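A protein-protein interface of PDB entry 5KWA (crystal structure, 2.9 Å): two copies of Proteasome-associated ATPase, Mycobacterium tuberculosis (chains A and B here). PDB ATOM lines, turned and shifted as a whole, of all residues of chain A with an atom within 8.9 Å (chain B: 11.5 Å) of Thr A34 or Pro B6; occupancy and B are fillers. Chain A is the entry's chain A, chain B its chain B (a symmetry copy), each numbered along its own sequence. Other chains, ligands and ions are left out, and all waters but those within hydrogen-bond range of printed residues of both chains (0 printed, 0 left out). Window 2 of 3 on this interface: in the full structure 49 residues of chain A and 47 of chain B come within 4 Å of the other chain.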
ATOM      1  N   ASP A  19     -29.488  -7.753  34.172  1.00  0.00           N
ATOM      2  CA  ASP A  19     -28.113  -8.151  33.859  1.00  0.00           C
ATOM      3  C   ASP A  19     -27.086  -6.988  33.722  1.00  0.00           C
ATOM      4  O   ASP A  19     -25.907  -7.248  33.468  1.00  0.00           O
ATOM      5  CB  ASP A  19     -28.146  -8.992  32.566  1.00  0.00           C
ATOM      6  CG  ASP A  19     -26.869  -9.779  32.328  1.00  0.00           C
ATOM      7  OD1 ASP A  19     -26.160  -9.480  31.342  1.00  0.00           O
ATOM      8  OD2 ASP A  19     -26.572 -10.695  33.124  1.00  0.00           O
ATOM      9  N   ASP A  20     -27.515  -5.729  33.896  1.00  0.00           N
ATOM     10  CA  ASP A  20     -26.666  -4.531  33.670  1.00  0.00           C
ATOM     11  C   ASP A  20     -26.185  -4.387  32.205  1.00  0.00           C
ATOM     12  O   ASP A  20     -25.163  -3.748  31.933  1.00  0.00           O
ATOM     13  CB  ASP A  20     -25.478  -4.462  34.677  1.00  0.00           C
ATOM     14  CG  ASP A  20     -25.715  -3.474  35.829  1.00  0.00           C
ATOM     15  OD1 ASP A  20     -26.307  -2.393  35.609  1.00  0.00           O
ATOM     16  OD2 ASP A  20     -25.275  -3.775  36.962  1.00  0.00           O
ATOM     17  N   THR A  21     -26.955  -4.958  31.273  1.00  0.00           N
ATOM     18  CA  THR A  21     -26.684  -4.891  29.834  1.00  0.00           C
ATOM     19  C   THR A  21     -27.855  -4.197  29.142  1.00  0.00           C
ATOM     20  O   THR A  21     -28.905  -3.952  29.757  1.00  0.00           O
ATOM     21  CB  THR A  21     -26.460  -6.295  29.219  1.00  0.00           C
ATOM     22  OG1 THR A  21     -27.452  -7.207  29.707  1.00  0.00           O
ATOM     23  CG2 THR A  21     -25.070  -6.823  29.561  1.00  0.00           C
ATOM     24  N   VAL A  22     -27.665  -3.889  27.860  1.00  0.00           N
ATOM     25  CA  VAL A  22     -28.612  -3.081  27.097  1.00  0.00           C
ATOM     26  C   VAL A  22     -28.859  -3.637  25.697  1.00  0.00           C
ATOM     27  O   VAL A  22     -27.938  -4.148  25.053  1.00  0.00           O
ATOM     28  CB  VAL A  22     -28.128  -1.616  26.974  1.00  0.00           C
ATOM     29  CG1 VAL A  22     -28.289  -0.886  28.299  1.00  0.00           C
ATOM     30  CG2 VAL A  22     -26.683  -1.529  26.491  1.00  0.00           C
ATOM     31  N   ASP A  23     -30.113  -3.532  25.249  1.00  0.00           N
ATOM     32  CA  ASP A  23     -30.475  -3.766  23.848  1.00  0.00           C
ATOM     33  C   ASP A  23     -30.256  -2.464  23.072  1.00  0.00           C
ATOM     34  O   ASP A  23     -30.862  -1.443  23.407  1.00  0.00           O
ATOM     35  CB  ASP A  23     -31.936  -4.231  23.708  1.00  0.00           C
ATOM     36  CG  ASP A  23     -32.109  -5.727  23.930  1.00  0.00           C
ATOM     37  OD1 ASP A  23     -31.437  -6.522  23.246  1.00  0.00           O
ATOM     38  OD2 ASP A  23     -32.940  -6.115  24.772  1.00  0.00           O
ATOM     39  N   VAL A  24     -29.389  -2.496  22.058  1.00  0.00           N
ATOM     40  CA  VAL A  24     -29.053  -1.300  21.271  1.00  0.00           C
ATOM     41  C   VAL A  24     -29.196  -1.569  19.775  1.00  0.00           C
ATOM     42  O   VAL A  24     -28.673  -2.566  19.270  1.00  0.00           O
ATOM     43  CB  VAL A  24     -27.624  -0.796  21.581  1.00  0.00           C
ATOM     44  CG1 VAL A  24     -27.164   0.262  20.579  1.00  0.00           C
ATOM     45  CG2 VAL A  24     -27.567  -0.235  22.995  1.00  0.00           C
ATOM     46  N   MET A  31     -28.961  -5.418  18.950  1.00  0.00           N
ATOM     47  CA  MET A  31     -27.846  -6.051  19.678  1.00  0.00           C
ATOM     48  C   MET A  31     -28.081  -6.061  21.189  1.00  0.00           C
ATOM     49  O   MET A  31     -28.789  -5.201  21.705  1.00  0.00           O
ATOM     50  CB  MET A  31     -26.550  -5.266  19.439  1.00  0.00           C
ATOM     51  CG  MET A  31     -26.152  -5.030  17.990  1.00  0.00           C
ATOM     52  SD  MET A  31     -25.063  -6.299  17.329  1.00  0.00           S
ATOM     53  CE  MET A  31     -24.114  -5.323  16.166  1.00  0.00           C
ATOM     54  N   ARG A  32     -27.468  -7.027  21.883  1.00  0.00           N
ATOM     55  CA  ARG A  32     -27.279  -6.982  23.345  1.00  0.00           C
ATOM     56  C   ARG A  32     -25.824  -6.605  23.588  1.00  0.00           C
ATOM     57  O   ARG A  32     -24.924  -7.332  23.160  1.00  0.00           O
ATOM     58  CB  ARG A  32     -27.586  -8.337  24.005  1.00  0.00           C
ATOM     59  CG  ARG A  32     -28.978  -8.446  24.613  1.00  0.00           C
ATOM     60  CD  ARG A  32     -29.017  -8.324  26.134  1.00  0.00           C
ATOM     61  NE  ARG A  32     -29.089  -9.634  26.795  1.00  0.00           N
ATOM     62  CZ  ARG A  32     -29.322  -9.832  28.098  1.00  0.00           C
ATOM     63  NH1 ARG A  32     -29.501  -8.809  28.936  1.00  0.00           N
ATOM     64  NH2 ARG A  32     -29.370 -11.074  28.571  1.00  0.00           N
ATOM     65  N   LEU A  33     -25.599  -5.476  24.259  1.00  0.00           N
ATOM     66  CA  LEU A  33     -24.247  -4.958  24.500  1.00  0.00           C
ATOM     67  C   LEU A  33     -24.008  -4.686  25.986  1.00  0.00           C
ATOM     68  O   LEU A  33     -24.947  -4.397  26.737  1.00  0.00           O
ATOM     69  CB  LEU A  33     -24.018  -3.670  23.702  1.00  0.00           C
ATOM     70  CG  LEU A  33     -24.370  -3.675  22.209  1.00  0.00           C
ATOM     71  CD1 LEU A  33     -24.150  -2.284  21.631  1.00  0.00           C
ATOM     72  CD2 LEU A  33     -23.571  -4.705  21.422  1.00  0.00           C
ATOM     73  N   THR A  34     -22.741  -4.786  26.394  1.00  0.00           N
ATOM     74  CA  THR A  34     -22.312  -4.488  27.762  1.00  0.00           C
ATOM     75  C   THR A  34     -21.980  -3.005  27.880  1.00  0.00           C
ATOM     76  O   THR A  34     -21.311  -2.451  27.007  1.00  0.00           O
ATOM     77  CB  THR A  34     -21.054  -5.292  28.142  1.00  0.00           C
ATOM     78  OG1 THR A  34     -20.074  -5.158  27.105  1.00  0.00           O
ATOM     79  CG2 THR A  34     -21.384  -6.767  28.328  1.00  0.00           C
ATOM     80  N   CYS A  35     -22.461  -2.367  28.946  1.00  0.00           N
ATOM     81  CA  CYS A  35     -22.062  -0.994  29.273  1.00  0.00           C
ATOM     82  C   CYS A  35     -20.650  -1.005  29.844  1.00  0.00           C
ATOM     83  O   CYS A  35     -20.259  -1.968  30.511  1.00  0.00           O
ATOM     84  CB  CYS A  35     -23.016  -0.367  30.292  1.00  0.00           C
ATOM     85  SG  CYS A  35     -24.698  -0.102  29.698  1.00  0.00           S
ATOM     86  N   SER A  36     -19.891   0.063  29.593  1.00  0.00           N
ATOM     87  CA  SER A  36     -18.539   0.186  30.149  1.00  0.00           C
ATOM     88  C   SER A  36     -18.641   0.432  31.660  1.00  0.00           C
ATOM     89  O   SER A  36     -19.686   0.899  32.137  1.00  0.00           O
ATOM     90  CB  SER A  36     -17.742   1.310  29.470  1.00  0.00           C
ATOM     91  OG  SER A  36     -18.012   2.577  30.051  1.00  0.00           O
ATOM     92  N   PRO A  37     -17.562   0.128  32.419  1.00  0.00           N
ATOM     93  CA  PRO A  37     -17.608   0.335  33.875  1.00  0.00           C
ATOM     94  C   PRO A  37     -17.936   1.783  34.278  1.00  0.00           C
ATOM     95  O   PRO A  37     -18.611   2.005  35.286  1.00  0.00           O
ATOM     96  CB  PRO A  37     -16.195  -0.058  34.337  1.00  0.00           C
ATOM     97  CG  PRO A  37     -15.618  -0.868  33.227  1.00  0.00           C
ATOM     98  CD  PRO A  37     -16.228  -0.326  31.975  1.00  0.00           C
ATOM     99  N   ILE A  39     -19.997   3.882  32.818  1.00  0.00           N
ATOM    100  CA  ILE A  39     -21.421   4.196  32.638  1.00  0.00           C
ATOM    101  C   ILE A  39     -22.317   3.477  33.653  1.00  0.00           C
ATOM    102  O   ILE A  39     -22.143   2.289  33.924  1.00  0.00           O
ATOM    103  CB  ILE A  39     -21.870   3.907  31.171  1.00  0.00           C
ATOM    104  CG1 ILE A  39     -21.407   5.042  30.234  1.00  0.00           C
ATOM    105  CG2 ILE A  39     -23.379   3.688  31.040  1.00  0.00           C
ATOM    106  CD1 ILE A  39     -22.018   6.414  30.493  1.00  0.00           C
ATOM    107  N   ALA A  41     -25.823   2.107  34.030  1.00  0.00           N
ATOM    108  CA  ALA A  41     -26.907   1.664  33.129  1.00  0.00           C
ATOM    109  C   ALA A  41     -28.336   1.969  33.609  1.00  0.00           C
ATOM    110  O   ALA A  41     -29.261   2.000  32.796  1.00  0.00           O
ATOM    111  CB  ALA A  41     -26.769   0.176  32.823  1.00  0.00           C
ATOM    112  N   LEU A  44     -29.826   5.437  32.258  1.00  0.00           N
ATOM    113  CA  LEU A  44     -30.151   5.511  30.825  1.00  0.00           C
ATOM    114  C   LEU A  44     -31.653   5.396  30.597  1.00  0.00           C
ATOM    115  O   LEU A  44     -32.368   4.793  31.401  1.00  0.00           O
ATOM    116  CB  LEU A  44     -29.422   4.428  30.020  1.00  0.00           C
ATOM    117  CG  LEU A  44     -27.892   4.355  30.114  1.00  0.00           C
ATOM    118  CD1 LEU A  44     -27.325   3.673  28.877  1.00  0.00           C
ATOM    119  CD2 LEU A  44     -27.245   5.725  30.298  1.00  0.00           C
ATOM    120  N   VAL A  50     -26.588   6.256  22.077  1.00  0.00           N
ATOM    121  CA  VAL A  50     -25.428   5.797  22.843  1.00  0.00           C
ATOM    122  C   VAL A  50     -24.237   5.655  21.906  1.00  0.00           C
ATOM    123  O   VAL A  50     -24.407   5.229  20.763  1.00  0.00           O
ATOM    124  CB  VAL A  50     -25.707   4.465  23.586  1.00  0.00           C
ATOM    125  CG1 VAL A  50     -26.773   4.671  24.647  1.00  0.00           C
ATOM    126  CG2 VAL A  50     -26.118   3.340  22.642  1.00  0.00           C
ATOM    127  N   ARG A  51     -23.047   6.033  22.386  1.00  0.00           N
ATOM    128  CA  ARG A  51     -21.796   5.856  21.633  1.00  0.00           C
ATOM    129  C   ARG A  51     -21.157   4.504  21.957  1.00  0.00           C
ATOM    130  O   ARG A  51     -21.386   3.951  23.036  1.00  0.00           O
ATOM    131  CB  ARG A  51     -20.808   6.998  21.915  1.00  0.00           C
ATOM    132  CG  ARG A  51     -19.724   7.119  20.846  1.00  0.00           C
ATOM    133  CD  ARG A  51     -18.967   8.441  20.853  1.00  0.00           C
ATOM    134  NE  ARG A  51     -17.720   8.376  21.617  1.00  0.00           N
ATOM    135  CZ  ARG A  51     -17.572   8.687  22.906  1.00  0.00           C
ATOM    136  NH1 ARG A  51     -18.591   9.110  23.650  1.00  0.00           N
ATOM    137  NH2 ARG A  51     -16.373   8.572  23.468  1.00  0.00           N
ATOM    138  N   LEU A  52     -20.371   3.983  21.011  1.00  0.00           N
ATOM    139  CA  LEU A  52     -19.753   2.653  21.116  1.00  0.00           C
ATOM    140  C   LEU A  52     -18.227   2.682  20.859  1.00  0.00           C
ATOM    141  O   LEU A  52     -17.619   3.748  20.830  1.00  0.00           O
ATOM    142  CB  LEU A  52     -20.440   1.690  20.128  1.00  0.00           C
ATOM    143  CG  LEU A  52     -21.975   1.559  20.069  1.00  0.00           C
ATOM    144  CD1 LEU A  52     -22.325   0.340  19.220  1.00  0.00           C
ATOM    145  CD2 LEU A  52     -22.643   1.464  21.440  1.00  0.00           C
ATOM    146  N   ASN A  53     -17.618   1.497  20.749  1.00  0.00           N
ATOM    147  CA  ASN A  53     -16.276   1.303  20.162  1.00  0.00           C
ATOM    148  C   ASN A  53     -16.326   0.040  19.287  1.00  0.00           C
ATOM    149  O   ASN A  53     -17.395  -0.570  19.166  1.00  0.00           O
ATOM    150  CB  ASN A  53     -15.202   1.195  21.257  1.00  0.00           C
ATOM    151  CG  ASN A  53     -15.426   0.020  22.202  1.00  0.00           C
ATOM    152  OD1 ASN A  53     -16.558  -0.415  22.425  1.00  0.00           O
ATOM    153  ND2 ASN A  53     -14.341  -0.488  22.774  1.00  0.00           N
ATOM    154  N   ALA A  55     -15.206  -2.904  19.878  1.00  0.00           N
ATOM    155  CA  ALA A  55     -15.643  -4.025  20.729  1.00  0.00           C
ATOM    156  C   ALA A  55     -17.169  -4.050  20.932  1.00  0.00           C
ATOM    157  O   ALA A  55     -17.705  -5.045  21.432  1.00  0.00           O
ATOM    158  CB  ALA A  55     -14.937  -3.981  22.078  1.00  0.00           C
ATOM    159  N   LEU A  56     -17.842  -2.952  20.565  1.00  0.00           N
ATOM    160  CA  LEU A  56     -19.301  -2.794  20.637  1.00  0.00           C
ATOM    161  C   LEU A  56     -19.734  -2.849  22.100  1.00  0.00           C
ATOM    162  O   LEU A  56     -20.440  -3.751  22.544  1.00  0.00           O
ATOM    163  CB  LEU A  56     -20.039  -3.797  19.727  1.00  0.00           C
ATOM    164  CG  LEU A  56     -19.686  -3.712  18.227  1.00  0.00           C
ATOM    165  CD1 LEU A  56     -20.201  -4.923  17.458  1.00  0.00           C
ATOM    166  CD2 LEU A  56     -20.202  -2.425  17.591  1.00  0.00           C
ATOM    167  N   THR A  57     -19.248  -1.854  22.832  1.00  0.00           N
ATOM    168  CA  THR A  57     -19.453  -1.704  24.264  1.00  0.00           C
ATOM    169  C   THR A  57     -19.859  -0.253  24.480  1.00  0.00           C
ATOM    170  O   THR A  57     -19.204   0.652  23.953  1.00  0.00           O
ATOM    171  CB  THR A  57     -18.139  -1.998  25.020  1.00  0.00           C
ATOM    172  OG1 THR A  57     -17.614  -3.259  24.583  1.00  0.00           O
ATOM    173  CG2 THR A  57     -18.335  -2.020  26.537  1.00  0.00           C
ATOM    174  N   VAL A  58     -20.925  -0.030  25.249  1.00  0.00           N
ATOM    175  CA  VAL A  58     -21.489   1.316  25.422  1.00  0.00           C
ATOM    176  C   VAL A  58     -20.585   2.169  26.307  1.00  0.00           C
ATOM    177  O   VAL A  58     -20.427   1.890  27.494  1.00  0.00           O
ATOM    178  CB  VAL A  58     -22.925   1.273  25.996  1.00  0.00           C
ATOM    179  CG1 VAL A  58     -23.427   2.672  26.350  1.00  0.00           C
ATOM    180  CG2 VAL A  58     -23.860   0.605  24.998  1.00  0.00           C
ATOM    181  N   VAL A  59     -20.016   3.214  25.711  1.00  0.00           N
ATOM    182  CA  VAL A  59     -19.053   4.088  26.379  1.00  0.00           C
ATOM    183  C   VAL A  59     -19.659   5.413  26.881  1.00  0.00           C
ATOM    184  O   VAL A  59     -19.139   5.995  27.831  1.00  0.00           O
ATOM    185  CB  VAL A  59     -17.817   4.363  25.472  1.00  0.00           C
ATOM    186  CG1 VAL A  59     -17.342   3.074  24.799  1.00  0.00           C
ATOM    187  CG2 VAL A  59     -18.095   5.446  24.428  1.00  0.00           C
ATOM    188  N   GLU A  60     -20.730   5.897  26.246  1.00  0.00           N
ATOM    189  CA  GLU A  60     -21.356   7.172  26.643  1.00  0.00           C
ATOM    190  C   GLU A  60     -22.839   7.255  26.263  1.00  0.00           C
ATOM    191  O   GLU A  60     -23.246   6.763  25.210  1.00  0.00           O
ATOM    192  CB  GLU A  60     -20.599   8.360  26.027  1.00  0.00           C
ATOM    193  CG  GLU A  60     -21.137   9.734  26.429  1.00  0.00           C
ATOM    194  CD  GLU A  60     -20.155  10.872  26.192  1.00  0.00           C
ATOM    195  OE1 GLU A  60     -19.759  11.099  25.026  1.00  0.00           O
ATOM    196  OE2 GLU A  60     -19.793  11.554  27.175  1.00  0.00           O
ATOM    197  N   PRO B   6     -19.835  -9.901  26.580  1.00  0.00           N
ATOM    198  CA  PRO B   6     -20.348 -10.849  25.588  1.00  0.00           C
ATOM    199  C   PRO B   6     -21.319 -10.195  24.570  1.00  0.00           C
ATOM    200  O   PRO B   6     -22.539 -10.288  24.740  1.00  0.00           O
ATOM    201  CB  PRO B   6     -21.045 -11.911  26.459  1.00  0.00           C
ATOM    202  CG  PRO B   6     -20.325 -11.868  27.772  1.00  0.00           C
ATOM    203  CD  PRO B   6     -19.655 -10.523  27.906  1.00  0.00           C
ATOM    204  N   PRO B   7     -20.783  -9.536  23.516  1.00  0.00           N
ATOM    205  CA  PRO B   7     -21.626  -8.784  22.565  1.00  0.00           C
ATOM    206  C   PRO B   7     -22.399  -9.705  21.615  1.00  0.00           C
ATOM    207  O   PRO B   7     -21.780 -10.484  20.890  1.00  0.00           O
ATOM    208  CB  PRO B   7     -20.609  -7.933  21.797  1.00  0.00           C
ATOM    209  CG  PRO B   7     -19.352  -8.734  21.827  1.00  0.00           C
ATOM    210  CD  PRO B   7     -19.365  -9.546  23.098  1.00  0.00           C
ATOM    211  N   SER B   8     -23.731  -9.590  21.609  1.00  0.00           N
ATOM    212  CA  SER B   8     -24.618 -10.577  20.960  1.00  0.00           C
ATOM    213  C   SER B   8     -25.735  -9.970  20.085  1.00  0.00           C
ATOM    214  O   SER B   8     -26.237  -8.880  20.377  1.00  0.00           O
ATOM    215  CB  SER B   8     -25.241 -11.484  22.031  1.00  0.00           C
ATOM    216  OG  SER B   8     -25.563 -10.769  23.208  1.00  0.00           O
ATOM    217  N   GLY B   9     -26.113 -10.700  19.027  1.00  0.00           N
ATOM    218  CA  GLY B   9     -27.197 -10.319  18.099  1.00  0.00           C
ATOM    219  C   GLY B   9     -28.446 -11.182  18.252  1.00  0.00           C
ATOM    220  O   GLY B   9     -28.463 -12.123  19.047  1.00  0.00           O
ATOM    221  N   TYR B  10     -29.489 -10.861  17.483  1.00  0.00           N
ATOM    222  CA  TYR B  10     -30.799 -11.529  17.586  1.00  0.00           C
ATOM    223  C   TYR B  10     -31.302 -12.082  16.241  1.00  0.00           C
ATOM    224  O   TYR B  10     -30.719 -11.831  15.170  1.00  0.00           O
ATOM    225  CB  TYR B  10     -31.847 -10.553  18.131  1.00  0.00           C
ATOM    226  CG  TYR B  10     -31.779 -10.247  19.611  1.00  0.00           C
ATOM    227  CD1 TYR B  10     -30.941  -9.243  20.098  1.00  0.00           C
ATOM    228  CD2 TYR B  10     -32.595 -10.918  20.523  1.00  0.00           C
ATOM    229  CE1 TYR B  10     -30.896  -8.935  21.451  1.00  0.00           C
ATOM    230  CE2 TYR B  10     -32.558 -10.616  21.882  1.00  0.00           C
ATOM    231  CZ  TYR B  10     -31.707  -9.622  22.341  1.00  0.00           C
ATOM    232  OH  TYR B  10     -31.670  -9.316  23.682  1.00  0.00           O
ATOM    233  N   ARG B  51     -31.708 -15.130  21.071  1.00  0.00           N
ATOM    234  CA  ARG B  51     -30.424 -14.423  21.143  1.00  0.00           C
ATOM    235  C   ARG B  51     -29.284 -15.319  20.660  1.00  0.00           C
ATOM    236  O   ARG B  51     -29.321 -16.534  20.864  1.00  0.00           O
ATOM    237  CB  ARG B  51     -30.150 -13.936  22.568  1.00  0.00           C
ATOM    238  CG  ARG B  51     -28.990 -12.953  22.658  1.00  0.00           C
ATOM    239  CD  ARG B  51     -29.108 -12.014  23.849  1.00  0.00           C
ATOM    240  NE  ARG B  51     -28.989 -12.714  25.125  1.00  0.00           N
ATOM    241  CZ  ARG B  51     -27.849 -13.163  25.657  1.00  0.00           C
ATOM    242  NH1 ARG B  51     -26.679 -13.012  25.034  1.00  0.00           N
ATOM    243  NH2 ARG B  51     -27.881 -13.782  26.830  1.00  0.00           N
ATOM    244  N   LEU B  52     -28.282 -14.701  20.031  1.00  0.00           N
ATOM    245  CA  LEU B  52     -27.187 -15.406  19.345  1.00  0.00           C
ATOM    246  C   LEU B  52     -25.799 -14.968  19.870  1.00  0.00           C
ATOM    247  O   LEU B  52     -25.713 -14.161  20.792  1.00  0.00           O
ATOM    248  CB  LEU B  52     -27.306 -15.161  17.828  1.00  0.00           C
ATOM    249  CG  LEU B  52     -28.201 -16.093  16.998  1.00  0.00           C
ATOM    250  CD1 LEU B  52     -29.626 -16.203  17.522  1.00  0.00           C
ATOM    251  CD2 LEU B  52     -28.201 -15.610  15.558  1.00  0.00           C
ATOM    252  N   ASN B  53     -24.729 -15.543  19.308  1.00  0.00           N
ATOM    253  CA  ASN B  53     -23.338 -15.101  19.552  1.00  0.00           C
ATOM    254  C   ASN B  53     -22.533 -15.213  18.246  1.00  0.00           C
ATOM    255  O   ASN B  53     -23.097 -15.599  17.219  1.00  0.00           O
ATOM    256  CB  ASN B  53     -22.697 -15.903  20.698  1.00  0.00           C
ATOM    257  CG  ASN B  53     -22.377 -17.335  20.313  1.00  0.00           C
ATOM    258  OD1 ASN B  53     -21.373 -17.608  19.652  1.00  0.00           O
ATOM    259  ND2 ASN B  53     -23.219 -18.261  20.746  1.00  0.00           N
ATOM    260  N   GLU B  54     -21.231 -14.911  18.271  1.00  0.00           N
ATOM    261  CA  GLU B  54     -20.437 -14.842  17.025  1.00  0.00           C
ATOM    262  C   GLU B  54     -20.114 -16.207  16.374  1.00  0.00           C
ATOM    263  O   GLU B  54     -19.637 -16.252  15.238  1.00  0.00           O
ATOM    264  CB  GLU B  54     -19.160 -14.010  17.218  1.00  0.00           C
ATOM    265  CG  GLU B  54     -18.670 -13.358  15.923  1.00  0.00           C
ATOM    266  CD  GLU B  54     -17.572 -12.327  16.112  1.00  0.00           C
ATOM    267  OE1 GLU B  54     -16.925 -11.974  15.099  1.00  0.00           O
ATOM    268  OE2 GLU B  54     -17.354 -11.858  17.253  1.00  0.00           O
ATOM    269  N   ALA B  55     -20.372 -17.303  17.084  1.00  0.00           N
ATOM    270  CA  ALA B  55     -20.433 -18.629  16.464  1.00  0.00           C
ATOM    271  C   ALA B  55     -21.827 -18.933  15.894  1.00  0.00           C
ATOM    272  O   ALA B  55     -22.005 -19.957  15.234  1.00  0.00           O
ATOM    273  CB  ALA B  55     -20.029 -19.697  17.466  1.00  0.00           C
ATOM    274  N   THR B  57     -24.936 -19.386  17.645  1.00  0.00           N
ATOM    275  CA  THR B  57     -25.525 -20.460  18.435  1.00  0.00           C
ATOM    276  C   THR B  57     -26.617 -19.837  19.290  1.00  0.00           C
ATOM    277  O   THR B  57     -26.388 -18.808  19.925  1.00  0.00           O
ATOM    278  CB  THR B  57     -24.459 -21.121  19.338  1.00  0.00           C
ATOM    279  OG1 THR B  57     -23.278 -21.384  18.570  1.00  0.00           O
ATOM    280  CG2 THR B  57     -24.966 -22.426  19.962  1.00  0.00           C
ATOM    281  N   VAL B  59     -28.309 -18.981  22.200  1.00  0.00           N
ATOM    282  CA  VAL B  59     -27.964 -18.990  23.623  1.00  0.00           C
ATOM    283  C   VAL B  59     -29.194 -18.811  24.543  1.00  0.00           C
ATOM    284  O   VAL B  59     -29.301 -19.499  25.559  1.00  0.00           O
ATOM    285  CB  VAL B  59     -26.836 -17.966  23.956  1.00  0.00           C
ATOM    286  CG1 VAL B  59     -25.685 -18.090  22.964  1.00  0.00           C
ATOM    287  CG2 VAL B  59     -27.347 -16.528  24.009  1.00  0.00           C
ATOM    288  N   GLU B  60     -30.120 -17.920  24.175  1.00  0.00           N
ATOM    289  CA  GLU B  60     -31.250 -17.530  25.044  1.00  0.00           C
ATOM    290  C   GLU B  60     -32.549 -17.360  24.243  1.00  0.00           C
ATOM    291  O   GLU B  60     -32.510 -17.009  23.060  1.00  0.00           O
ATOM    292  CB  GLU B  60     -30.902 -16.223  25.774  1.00  0.00           C
ATOM    293  CG  GLU B  60     -31.960 -15.702  26.745  1.00  0.00           C
ATOM    294  CD  GLU B  60     -31.496 -14.487  27.541  1.00  0.00           C
ATOM    295  OE1 GLU B  60     -31.875 -14.369  28.727  1.00  0.00           O
ATOM    296  OE2 GLU B  60     -30.756 -13.643  26.989  1.00  0.00           O
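OD1 of Asp A23 is in hydrogen-bond range of OH of Tyr B10. N of Arg A32 is in hydrogen-bond range of O of Ser B8 (2.7 Å). The guanidinium group of Arg A32 lies within salt-bridge range of the side-chain carboxylate of Glu B60 (3.3 Å).
Among the printed residues, merely in contact across the chains: Met A31 with Ser B8, Arg A32 with Pro B7, Arg A32 with Tyr B10, Arg A32 with Arg B51 and Thr A34 with Pro B6.
Positions printed for both chains: 51, 52, 53, 55, 57, 59 and 60. Of the 8 pairs that touch across the chains among the printed residues, none has its exchanged pair printed and touching as well.
Thr A34 touches just one residue of chain B: Pro B6 (3.9 Å). Pro B6 touches just one residue of chain A: Thr A34 (3.9 Å). No residue of chain B comes within 4 Å of Ser A36. No residue of chain B comes within 4 Å of Thr A57. Printed residues of chain A within 4 Å of Pro B7: Arg A32 (3.7 Å). Of the printed residues of chain B, Arg A32 touches Pro B7, Ser B8, Tyr B10, Arg B51 and Glu B60. Of the printed residues of chain A, Ser B8 touches Met A31 (3.3 Å) and Arg A32 (2.7 Å). Of the printed residues of chain B, Met A31 touches Ser B8 (3.3 Å). Printed residues of chain A within 4 Å of Arg B51: Arg A32 (3.5 Å). Thr B57 touches none of the printed residues of chain A. The nearest residue of chain B that does not touch Thr A34 is Pro B7 (5.6 Å).
OG1 of Thr A21 lies within hydrogen-bond range of NH1 of Arg A32, 2.7 Å away. The backbone carbonyl oxygen (O) of Met A31 is in hydrogen-bond range of the backbone NH (N) of Val A24, 2.8 Å away. O of Pro B6 sits at hydrogen-bond distance from OG of Ser B8, at 3.4 Å. The guanidinium group of Arg B51 lies within hydrogen-bond range of the side-chain hydroxyl of Ser B8 (3.1 Å). The backbone carbonyl oxygen (O) of Arg B51 lies within hydrogen-bond range of the backbone NH (N) of Val B59. OE2 of Glu B60 lies within salt-bridge range of NE of Arg B51 (2.7 Å).
Of the 13 printed residues of chain B, 6 touch a printed residue of chain A. Hydrophobic or aromatic side chains of chain B that line the printed part of chain A: Tyr B10. Of the 26 printed residues of chain A, 4 touch a printed residue of chain B. Printed residues of chain A that touch a printed residue of chain B: Asp A23, Met A31, Arg A32 and Thr A34. Hydrophobic or aromatic side chains of chain A within 4 Å of the printed part of chain B: Met A31. Among the printed residues, 8 pairs touch across the chains.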
